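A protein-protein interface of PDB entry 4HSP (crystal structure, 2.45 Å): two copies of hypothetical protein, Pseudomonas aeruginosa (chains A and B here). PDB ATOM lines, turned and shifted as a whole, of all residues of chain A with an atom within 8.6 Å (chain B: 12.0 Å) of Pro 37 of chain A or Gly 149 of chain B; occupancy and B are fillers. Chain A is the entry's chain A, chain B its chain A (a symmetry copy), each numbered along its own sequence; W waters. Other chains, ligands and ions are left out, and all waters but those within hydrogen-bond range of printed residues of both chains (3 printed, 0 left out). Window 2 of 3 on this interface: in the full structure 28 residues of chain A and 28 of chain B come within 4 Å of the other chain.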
ATOM      1  N   ALA A  29     -16.837  17.664  18.310  1.00  0.00           N
ATOM      2  CA  ALA A  29     -17.676  18.780  18.766  1.00  0.00           C
ATOM      3  C   ALA A  29     -18.808  19.033  17.744  1.00  0.00           C
ATOM      4  O   ALA A  29     -19.953  19.244  18.154  1.00  0.00           O
ATOM      5  CB  ALA A  29     -16.835  20.035  18.958  1.00  0.00           C
ATOM      6  N   LEU A  32     -21.431  16.089  17.982  1.00  0.00           N
ATOM      7  CA  LEU A  32     -22.260  16.223  19.189  1.00  0.00           C
ATOM      8  C   LEU A  32     -23.198  17.421  19.085  1.00  0.00           C
ATOM      9  O   LEU A  32     -24.265  17.408  19.702  1.00  0.00           O
ATOM     10  CB  LEU A  32     -21.392  16.320  20.463  1.00  0.00           C
ATOM     11  CG  LEU A  32     -20.575  15.071  20.799  1.00  0.00           C
ATOM     12  CD1 LEU A  32     -19.678  15.304  21.965  1.00  0.00           C
ATOM     13  CD2 LEU A  32     -21.445  13.913  21.112  1.00  0.00           C
ATOM     14  N   SER A  33     -22.789  18.454  18.322  1.00  0.00           N
ATOM     15  CA  SER A  33     -23.574  19.649  18.028  1.00  0.00           C
ATOM     16  C   SER A  33     -24.723  19.276  17.108  1.00  0.00           C
ATOM     17  O   SER A  33     -25.867  19.637  17.402  1.00  0.00           O
ATOM     18  CB  SER A  33     -22.706  20.716  17.370  1.00  0.00           C
ATOM     19  OG  SER A  33     -22.128  21.601  18.311  1.00  0.00           O
ATOM     20  N   GLU A  34     -24.422  18.528  16.004  1.00  0.00           N
ATOM     21  CA  GLU A  34     -25.407  18.060  15.019  1.00  0.00           C
ATOM     22  C   GLU A  34     -26.400  17.105  15.685  1.00  0.00           C
ATOM     23  O   GLU A  34     -27.596  17.179  15.405  1.00  0.00           O
ATOM     24  CB  GLU A  34     -24.764  17.394  13.767  1.00  0.00           C
ATOM     25  CG  GLU A  34     -23.920  18.309  12.885  1.00  0.00           C
ATOM     26  CD  GLU A  34     -24.525  19.642  12.484  1.00  0.00           C
ATOM     27  OE1 GLU A  34     -25.423  19.649  11.609  1.00  0.00           O
ATOM     28  OE2 GLU A  34     -24.090  20.681  13.035  1.00  0.00           O
ATOM     29  N   ALA A  35     -25.907  16.236  16.584  1.00  0.00           N
ATOM     30  CA  ALA A  35     -26.744  15.324  17.362  1.00  0.00           C
ATOM     31  C   ALA A  35     -27.557  16.135  18.379  1.00  0.00           C
ATOM     32  O   ALA A  35     -27.175  17.258  18.729  1.00  0.00           O
ATOM     33  CB  ALA A  35     -25.886  14.285  18.067  1.00  0.00           C
ATOM     34  N   GLY A  36     -28.674  15.572  18.816  1.00  0.00           N
ATOM     35  CA  GLY A  36     -29.586  16.209  19.760  1.00  0.00           C
ATOM     36  C   GLY A  36     -28.994  16.651  21.086  1.00  0.00           C
ATOM     37  O   GLY A  36     -27.817  16.397  21.365  1.00  0.00           O
ATOM     38  N   PRO A  37     -29.814  17.323  21.936  1.00  0.00           N
ATOM     39  CA  PRO A  37     -29.314  17.752  23.263  1.00  0.00           C
ATOM     40  C   PRO A  37     -29.135  16.576  24.220  1.00  0.00           C
ATOM     41  O   PRO A  37     -28.502  16.724  25.272  1.00  0.00           O
ATOM     42  CB  PRO A  37     -30.397  18.705  23.766  1.00  0.00           C
ATOM     43  CG  PRO A  37     -31.636  18.262  23.070  1.00  0.00           C
ATOM     44  CD  PRO A  37     -31.234  17.684  21.744  1.00  0.00           C
ATOM     45  N   ALA A  38     -29.714  15.416  23.852  1.00  0.00           N
ATOM     46  CA  ALA A  38     -29.617  14.171  24.608  1.00  0.00           C
ATOM     47  C   ALA A  38     -28.181  13.625  24.534  1.00  0.00           C
ATOM     48  O   ALA A  38     -27.553  13.357  25.566  1.00  0.00           O
ATOM     49  CB  ALA A  38     -30.608  13.157  24.041  1.00  0.00           C
ATOM     50  N   ALA A  39     -27.650  13.586  23.298  1.00  0.00           N
ATOM     51  CA  ALA A  39     -26.340  13.086  22.902  1.00  0.00           C
ATOM     52  C   ALA A  39     -25.167  13.937  23.385  1.00  0.00           C
ATOM     53  O   ALA A  39     -24.047  13.450  23.329  1.00  0.00           O
ATOM     54  CB  ALA A  39     -26.278  12.952  21.389  1.00  0.00           C
ATOM     55  N   SER A  40     -25.399  15.171  23.870  1.00  0.00           N
ATOM     56  CA  SER A  40     -24.339  16.073  24.358  1.00  0.00           C
ATOM     57  C   SER A  40     -23.382  15.366  25.332  1.00  0.00           C
ATOM     58  O   SER A  40     -22.162  15.452  25.150  1.00  0.00           O
ATOM     59  CB  SER A  40     -24.943  17.289  25.053  1.00  0.00           C
ATOM     60  OG  SER A  40     -25.969  17.878  24.279  1.00  0.00           O
ATOM     61  N   GLN A  41     -23.936  14.669  26.356  1.00  0.00           N
ATOM     62  CA  GLN A  41     -23.143  13.978  27.382  1.00  0.00           C
ATOM     63  C   GLN A  41     -22.976  12.530  26.958  1.00  0.00           C
ATOM     64  O   GLN A  41     -23.937  11.763  26.974  1.00  0.00           O
ATOM     65  CB  GLN A  41     -23.788  14.121  28.776  1.00  0.00           C
ATOM     66  CG  GLN A  41     -23.051  13.385  29.890  1.00  0.00           C
ATOM     67  CD  GLN A  41     -23.761  13.560  31.193  1.00  0.00           C
ATOM     68  OE1 GLN A  41     -24.978  13.394  31.299  1.00  0.00           O
ATOM     69  NE2 GLN A  41     -23.019  13.915  32.211  1.00  0.00           N
ATOM     70  N   GLN A  42     -21.752  12.167  26.548  1.00  0.00           N
ATOM     71  CA  GLN A  42     -21.496  10.843  26.004  1.00  0.00           C
ATOM     72  C   GLN A  42     -21.386   9.737  27.040  1.00  0.00           C
ATOM     73  O   GLN A  42     -21.633   8.587  26.682  1.00  0.00           O
ATOM     74  CB  GLN A  42     -20.306  10.852  25.058  1.00  0.00           C
ATOM     75  CG  GLN A  42     -20.738  11.266  23.633  1.00  0.00           C
ATOM     76  CD  GLN A  42     -21.891  10.452  23.021  1.00  0.00           C
ATOM     77  OE1 GLN A  42     -21.750   9.277  22.644  1.00  0.00           O
ATOM     78  NE2 GLN A  42     -23.049  11.075  22.878  1.00  0.00           N
ATOM     79  N   CYS A  86     -20.782  22.042  29.744  1.00  0.00           N
ATOM     80  CA  CYS A  86     -22.202  21.982  29.359  1.00  0.00           C
ATOM     81  C   CYS A  86     -22.611  23.154  28.505  1.00  0.00           C
ATOM     82  O   CYS A  86     -23.632  23.060  27.836  1.00  0.00           O
ATOM     83  CB  CYS A  86     -23.132  21.843  30.563  1.00  0.00           C
ATOM     84  SG  CYS A  86     -22.685  20.502  31.697  1.00  0.00           S
ATOM     85  N   ILE A  87     -21.846  24.255  28.524  1.00  0.00           N
ATOM     86  CA  ILE A  87     -22.187  25.491  27.814  1.00  0.00           C
ATOM     87  C   ILE A  87     -21.333  25.700  26.568  1.00  0.00           C
ATOM     88  O   ILE A  87     -21.878  25.796  25.470  1.00  0.00           O
ATOM     89  CB  ILE A  87     -22.057  26.694  28.800  1.00  0.00           C
ATOM     90  CG1 ILE A  87     -23.056  26.565  29.976  1.00  0.00           C
ATOM     91  CG2 ILE A  87     -22.172  28.055  28.098  1.00  0.00           C
ATOM     92  CD1 ILE A  87     -22.376  26.298  31.276  1.00  0.00           C
ATOM     93  N   HIS A  88     -20.018  25.822  26.741  1.00  0.00           N
ATOM     94  CA  HIS A  88     -19.084  26.088  25.651  1.00  0.00           C
ATOM     95  C   HIS A  88     -18.490  24.811  25.059  1.00  0.00           C
ATOM     96  O   HIS A  88     -18.115  24.801  23.890  1.00  0.00           O
ATOM     97  CB  HIS A  88     -17.976  27.041  26.121  1.00  0.00           C
ATOM     98  CG  HIS A  88     -18.488  28.410  26.475  1.00  0.00           C
ATOM     99  ND1 HIS A  88     -18.123  29.036  27.659  1.00  0.00           N
ATOM    100  CD2 HIS A  88     -19.328  29.224  25.791  1.00  0.00           C
ATOM    101  CE1 HIS A  88     -18.745  30.200  27.653  1.00  0.00           C
ATOM    102  NE2 HIS A  88     -19.491  30.350  26.552  1.00  0.00           N
ATOM    103  N   VAL A  89     -18.439  23.743  25.846  1.00  0.00           N
ATOM    104  CA  VAL A  89     -17.959  22.421  25.448  1.00  0.00           C
ATOM    105  C   VAL A  89     -18.977  21.391  25.934  1.00  0.00           C
ATOM    106  O   VAL A  89     -19.725  21.710  26.862  1.00  0.00           O
ATOM    107  CB  VAL A  89     -16.534  22.110  26.021  1.00  0.00           C
ATOM    108  CG1 VAL A  89     -15.437  22.925  25.320  1.00  0.00           C
ATOM    109  CG2 VAL A  89     -16.486  22.292  27.537  1.00  0.00           C
ATOM    110  N   PRO A  90     -18.975  20.137  25.419  1.00  0.00           N
ATOM    111  CA  PRO A  90     -19.921  19.122  25.935  1.00  0.00           C
ATOM    112  C   PRO A  90     -19.813  18.845  27.439  1.00  0.00           C
ATOM    113  O   PRO A  90     -18.742  19.008  28.019  1.00  0.00           O
ATOM    114  CB  PRO A  90     -19.540  17.855  25.157  1.00  0.00           C
ATOM    115  CG  PRO A  90     -18.945  18.351  23.904  1.00  0.00           C
ATOM    116  CD  PRO A  90     -18.203  19.610  24.275  1.00  0.00           C
ATOM    117  N   PRO A  91     -20.908  18.389  28.090  1.00  0.00           N
ATOM    118  CA  PRO A  91     -20.822  18.051  29.525  1.00  0.00           C
ATOM    119  C   PRO A  91     -19.758  16.986  29.839  1.00  0.00           C
ATOM    120  O   PRO A  91     -19.548  16.075  29.015  1.00  0.00           O
ATOM    121  CB  PRO A  91     -22.211  17.469  29.833  1.00  0.00           C
ATOM    122  CG  PRO A  91     -23.082  17.947  28.783  1.00  0.00           C
ATOM    123  CD  PRO A  91     -22.264  18.138  27.561  1.00  0.00           C
ATOM    124  N   SER A 128     -30.603  16.365  35.091  1.00  0.00           N
ATOM    125  CA  SER A 128     -31.048  17.651  34.573  1.00  0.00           C
ATOM    126  C   SER A 128     -31.025  17.515  33.077  1.00  0.00           C
ATOM    127  O   SER A 128     -30.431  16.562  32.562  1.00  0.00           O
ATOM    128  CB  SER A 128     -30.182  18.808  35.078  1.00  0.00           C
ATOM    129  OG  SER A 128     -28.828  18.746  34.666  1.00  0.00           O
ATOM    130  N   GLU A 129     -31.688  18.417  32.373  1.00  0.00           N
ATOM    131  CA  GLU A 129     -31.721  18.367  30.917  1.00  0.00           C
ATOM    132  C   GLU A 129     -30.315  18.690  30.344  1.00  0.00           C
ATOM    133  O   GLU A 129     -29.974  18.271  29.233  1.00  0.00           O
ATOM    134  CB  GLU A 129     -32.778  19.341  30.408  1.00  0.00           C
ATOM    135  CG  GLU A 129     -33.442  18.946  29.108  1.00  0.00           C
ATOM    136  CD  GLU A 129     -34.621  19.842  28.783  1.00  0.00           C
ATOM    137  OE1 GLU A 129     -35.604  19.835  29.562  1.00  0.00           O
ATOM    138  OE2 GLU A 129     -34.541  20.591  27.782  1.00  0.00           O
ATOM    139  N   LEU A 130     -29.510  19.402  31.140  1.00  0.00           N
ATOM    140  CA  LEU A 130     -28.160  19.850  30.844  1.00  0.00           C
ATOM    141  C   LEU A 130     -27.164  18.723  30.958  1.00  0.00           C
ATOM    142  O   LEU A 130     -26.240  18.663  30.152  1.00  0.00           O
ATOM    143  CB  LEU A 130     -27.790  20.976  31.821  1.00  0.00           C
ATOM    144  CG  LEU A 130     -26.809  22.054  31.356  1.00  0.00           C
ATOM    145  CD1 LEU A 130     -27.246  22.718  30.034  1.00  0.00           C
ATOM    146  CD2 LEU A 130     -26.679  23.115  32.413  1.00  0.00           C
ATOM    147  N   ALA A 131     -27.303  17.862  31.990  1.00  0.00           N
ATOM    148  CA  ALA A 131     -26.405  16.748  32.253  1.00  0.00           C
ATOM    149  C   ALA A 131     -26.881  15.870  33.405  1.00  0.00           C
ATOM    150  O   ALA A 131     -27.584  16.328  34.296  1.00  0.00           O
ATOM    151  CB  ALA A 131     -25.015  17.274  32.574  1.00  0.00           C
ATOM    152  N   PRO B 114     -13.942  29.467  24.449  1.00  0.00           N
ATOM    153  CA  PRO B 114     -12.734  28.955  23.808  1.00  0.00           C
ATOM    154  C   PRO B 114     -12.717  29.372  22.344  1.00  0.00           C
ATOM    155  O   PRO B 114     -13.750  29.770  21.781  1.00  0.00           O
ATOM    156  CB  PRO B 114     -12.849  27.438  23.987  1.00  0.00           C
ATOM    157  CG  PRO B 114     -14.291  27.168  24.209  1.00  0.00           C
ATOM    158  CD  PRO B 114     -15.023  28.455  24.415  1.00  0.00           C
ATOM    159  N   TYR B 145     -14.695  28.739  19.208  1.00  0.00           N
ATOM    160  CA  TYR B 145     -14.936  27.297  19.243  1.00  0.00           C
ATOM    161  C   TYR B 145     -16.439  27.113  19.226  1.00  0.00           C
ATOM    162  O   TYR B 145     -17.139  27.570  20.138  1.00  0.00           O
ATOM    163  CB  TYR B 145     -14.292  26.694  20.503  1.00  0.00           C
ATOM    164  CG  TYR B 145     -14.357  25.190  20.634  1.00  0.00           C
ATOM    165  CD1 TYR B 145     -15.472  24.565  21.195  1.00  0.00           C
ATOM    166  CD2 TYR B 145     -13.251  24.399  20.336  1.00  0.00           C
ATOM    167  CE1 TYR B 145     -15.515  23.183  21.373  1.00  0.00           C
ATOM    168  CE2 TYR B 145     -13.270  23.017  20.541  1.00  0.00           C
ATOM    169  CZ  TYR B 145     -14.409  22.414  21.045  1.00  0.00           C
ATOM    170  OH  TYR B 145     -14.411  21.061  21.251  1.00  0.00           O
ATOM    171  N   GLU B 146     -16.945  26.510  18.163  1.00  0.00           N
ATOM    172  CA  GLU B 146     -18.375  26.358  18.027  1.00  0.00           C
ATOM    173  C   GLU B 146     -18.826  25.029  18.591  1.00  0.00           C
ATOM    174  O   GLU B 146     -18.266  23.959  18.264  1.00  0.00           O
ATOM    175  CB  GLU B 146     -18.816  26.517  16.569  1.00  0.00           C
ATOM    176  CG  GLU B 146     -18.694  27.942  16.029  1.00  0.00           C
ATOM    177  CD  GLU B 146     -19.746  28.975  16.420  1.00  0.00           C
ATOM    178  OE1 GLU B 146     -20.726  28.614  17.114  1.00  0.00           O
ATOM    179  OE2 GLU B 146     -19.591  30.151  16.015  1.00  0.00           O
ATOM    180  N   TYR B 147     -19.838  25.120  19.475  1.00  0.00           N
ATOM    181  CA  TYR B 147     -20.504  23.990  20.099  1.00  0.00           C
ATOM    182  C   TYR B 147     -21.874  24.423  20.592  1.00  0.00           C
ATOM    183  O   TYR B 147     -21.971  25.404  21.331  1.00  0.00           O
ATOM    184  CB  TYR B 147     -19.664  23.345  21.245  1.00  0.00           C
ATOM    185  CG  TYR B 147     -20.478  22.401  22.099  1.00  0.00           C
ATOM    186  CD1 TYR B 147     -20.787  21.117  21.654  1.00  0.00           C
ATOM    187  CD2 TYR B 147     -21.039  22.827  23.300  1.00  0.00           C
ATOM    188  CE1 TYR B 147     -21.605  20.270  22.399  1.00  0.00           C
ATOM    189  CE2 TYR B 147     -21.855  21.990  24.055  1.00  0.00           C
ATOM    190  CZ  TYR B 147     -22.121  20.704  23.610  1.00  0.00           C
ATOM    191  OH  TYR B 147     -22.898  19.865  24.379  1.00  0.00           O
ATOM    192  N   GLU B 148     -22.917  23.644  20.219  1.00  0.00           N
ATOM    193  CA  GLU B 148     -24.317  23.834  20.612  1.00  0.00           C
ATOM    194  C   GLU B 148     -24.800  22.665  21.505  1.00  0.00           C
ATOM    195  O   GLU B 148     -24.778  21.496  21.087  1.00  0.00           O
ATOM    196  CB  GLU B 148     -25.232  24.003  19.380  1.00  0.00           C
ATOM    197  CG  GLU B 148     -25.091  25.338  18.655  1.00  0.00           C
ATOM    198  CD  GLU B 148     -25.175  26.581  19.527  1.00  0.00           C
ATOM    199  OE1 GLU B 148     -26.229  26.793  20.169  1.00  0.00           O
ATOM    200  OE2 GLU B 148     -24.170  27.329  19.590  1.00  0.00           O
ATOM    201  N   GLY B 149     -25.204  23.009  22.732  1.00  0.00           N
ATOM    202  CA  GLY B 149     -25.693  22.072  23.732  1.00  0.00           C
ATOM    203  C   GLY B 149     -27.039  21.477  23.387  1.00  0.00           C
ATOM    204  O   GLY B 149     -27.220  20.266  23.502  1.00  0.00           O
HETATM  205  O   HOH W   1     -18.567  27.121  22.426  1.00  0.00           O
HETATM  206  O   HOH W   2     -21.507  27.697  22.811  1.00  0.00           O
HETATM  207  O   HOH W   3     -24.107  20.959  26.539  1.00  0.00           O
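O of Pro 114 of chain B lies within hydrogen-bond range of N of Tyr 145 of chain B (2.9 Å).
O of Pro 37 of chain A is in hydrogen-bond range of OG of Ser 40 of chain A (3.0 Å).
OG of Ser 33 of chain A lies within hydrogen-bond range of O of Ala 29 of chain A, at 3.2 Å.
Printed residues of chain A that touch a printed residue of chain B: Ala 29, Ser 33, Pro 37, Ser 40, Ile 87, His 88, Val 89, Pro 90 and Pro 91.
Among the printed residues, 14 pairs touch across the chains.
Water W3 lies within hydrogen-bond range of O of Cys 86 of chain A (2.5 Å) and OH of Tyr 147 of chain B (2.7 Å).
Water W1 bridges the backbone carbonyl oxygen (O) of Tyr 145 of chain B (2.7 Å) and the backbone carbonyl oxygen (O) of His 88 of chain A (2.8 Å).
Water W2 lies within hydrogen-bond range of O of Tyr 147 of chain B (2.8 Å) and O of Ile 87 of chain A (3.3 Å).
The side-chain hydroxyl (OG) of Ser 33 of chain A sits at hydrogen-bond distance from the backbone NH (N) of Glu 148 of chain B, at 2.9 Å.
The side-chain hydroxyl of Ser 40 of chain A sits at hydrogen-bond distance from the backbone carbonyl oxygen of Gly 149 of chain B.
Ala 29 of chain A touches Tyr 145 of chain B (CB to OH, 3.5 Å).
OG of Ser 33 of chain A touches CA of Tyr 147 of chain B (3.4 Å).
Ser 40 of chain A touches Tyr 147 of chain B.
CD2 of Tyr 147 of chain B touches O of Ile 87 of chain A, at 3.8 Å.
CD of Pro 114 of chain B touches CB of His 88 of chain A (3.7 Å).
His 88 of chain A touches Tyr 145 of chain B (O to CD1, 3.8 Å).
His 88 of chain A touches Tyr 147 of chain B (O to CB, 3.4 Å).
Tyr 145 of chain B touches Val 89 of chain A (CE1 to CG1, 3.96 Å).
Tyr 147 of chain B touches Val 89 of chain A (CE2 to C, 3.5 Å).
CD of Pro 91 of chain A touches OH of Tyr 147 of chain B, at 3.7 Å.
Ala 35 of chain A touches none of the printed residues of chain B.
Printed residues of chain B within 4 Å of Pro 37 of chain A: Gly 149 (3.3 Å).
No residue of chain B comes within 4 Å of Ala 39 of chain A.
Of chain B, only Tyr 147 (3.4 Å) and Gly 149 (2.8 Å) come within 4 Å of Ser 40 of chain A.
Printed residues of chain B within 4 Å of Ile 87 of chain A: Tyr 147.
Of the printed residues of chain B, His 88 of chain A touches Pro 114, Tyr 145 and Tyr 147.
Of the printed residues of chain B, Val 89 of chain A touches Tyr 145 (3.96 Å) and Tyr 147 (3.5 Å).
Ser 128 of chain A touches none of the printed residues of chain B.
Of the printed residues of chain A, Pro 114 of chain B touches His 88.
Printed residues of chain A within 4 Å of Tyr 145 of chain B: Ala 29, His 88 and Val 89.
The nearest printed residue of chain B that does not touch Ile 87 of chain A is Gly 149 of chain B (5.1 Å).
No position is printed for both chains.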
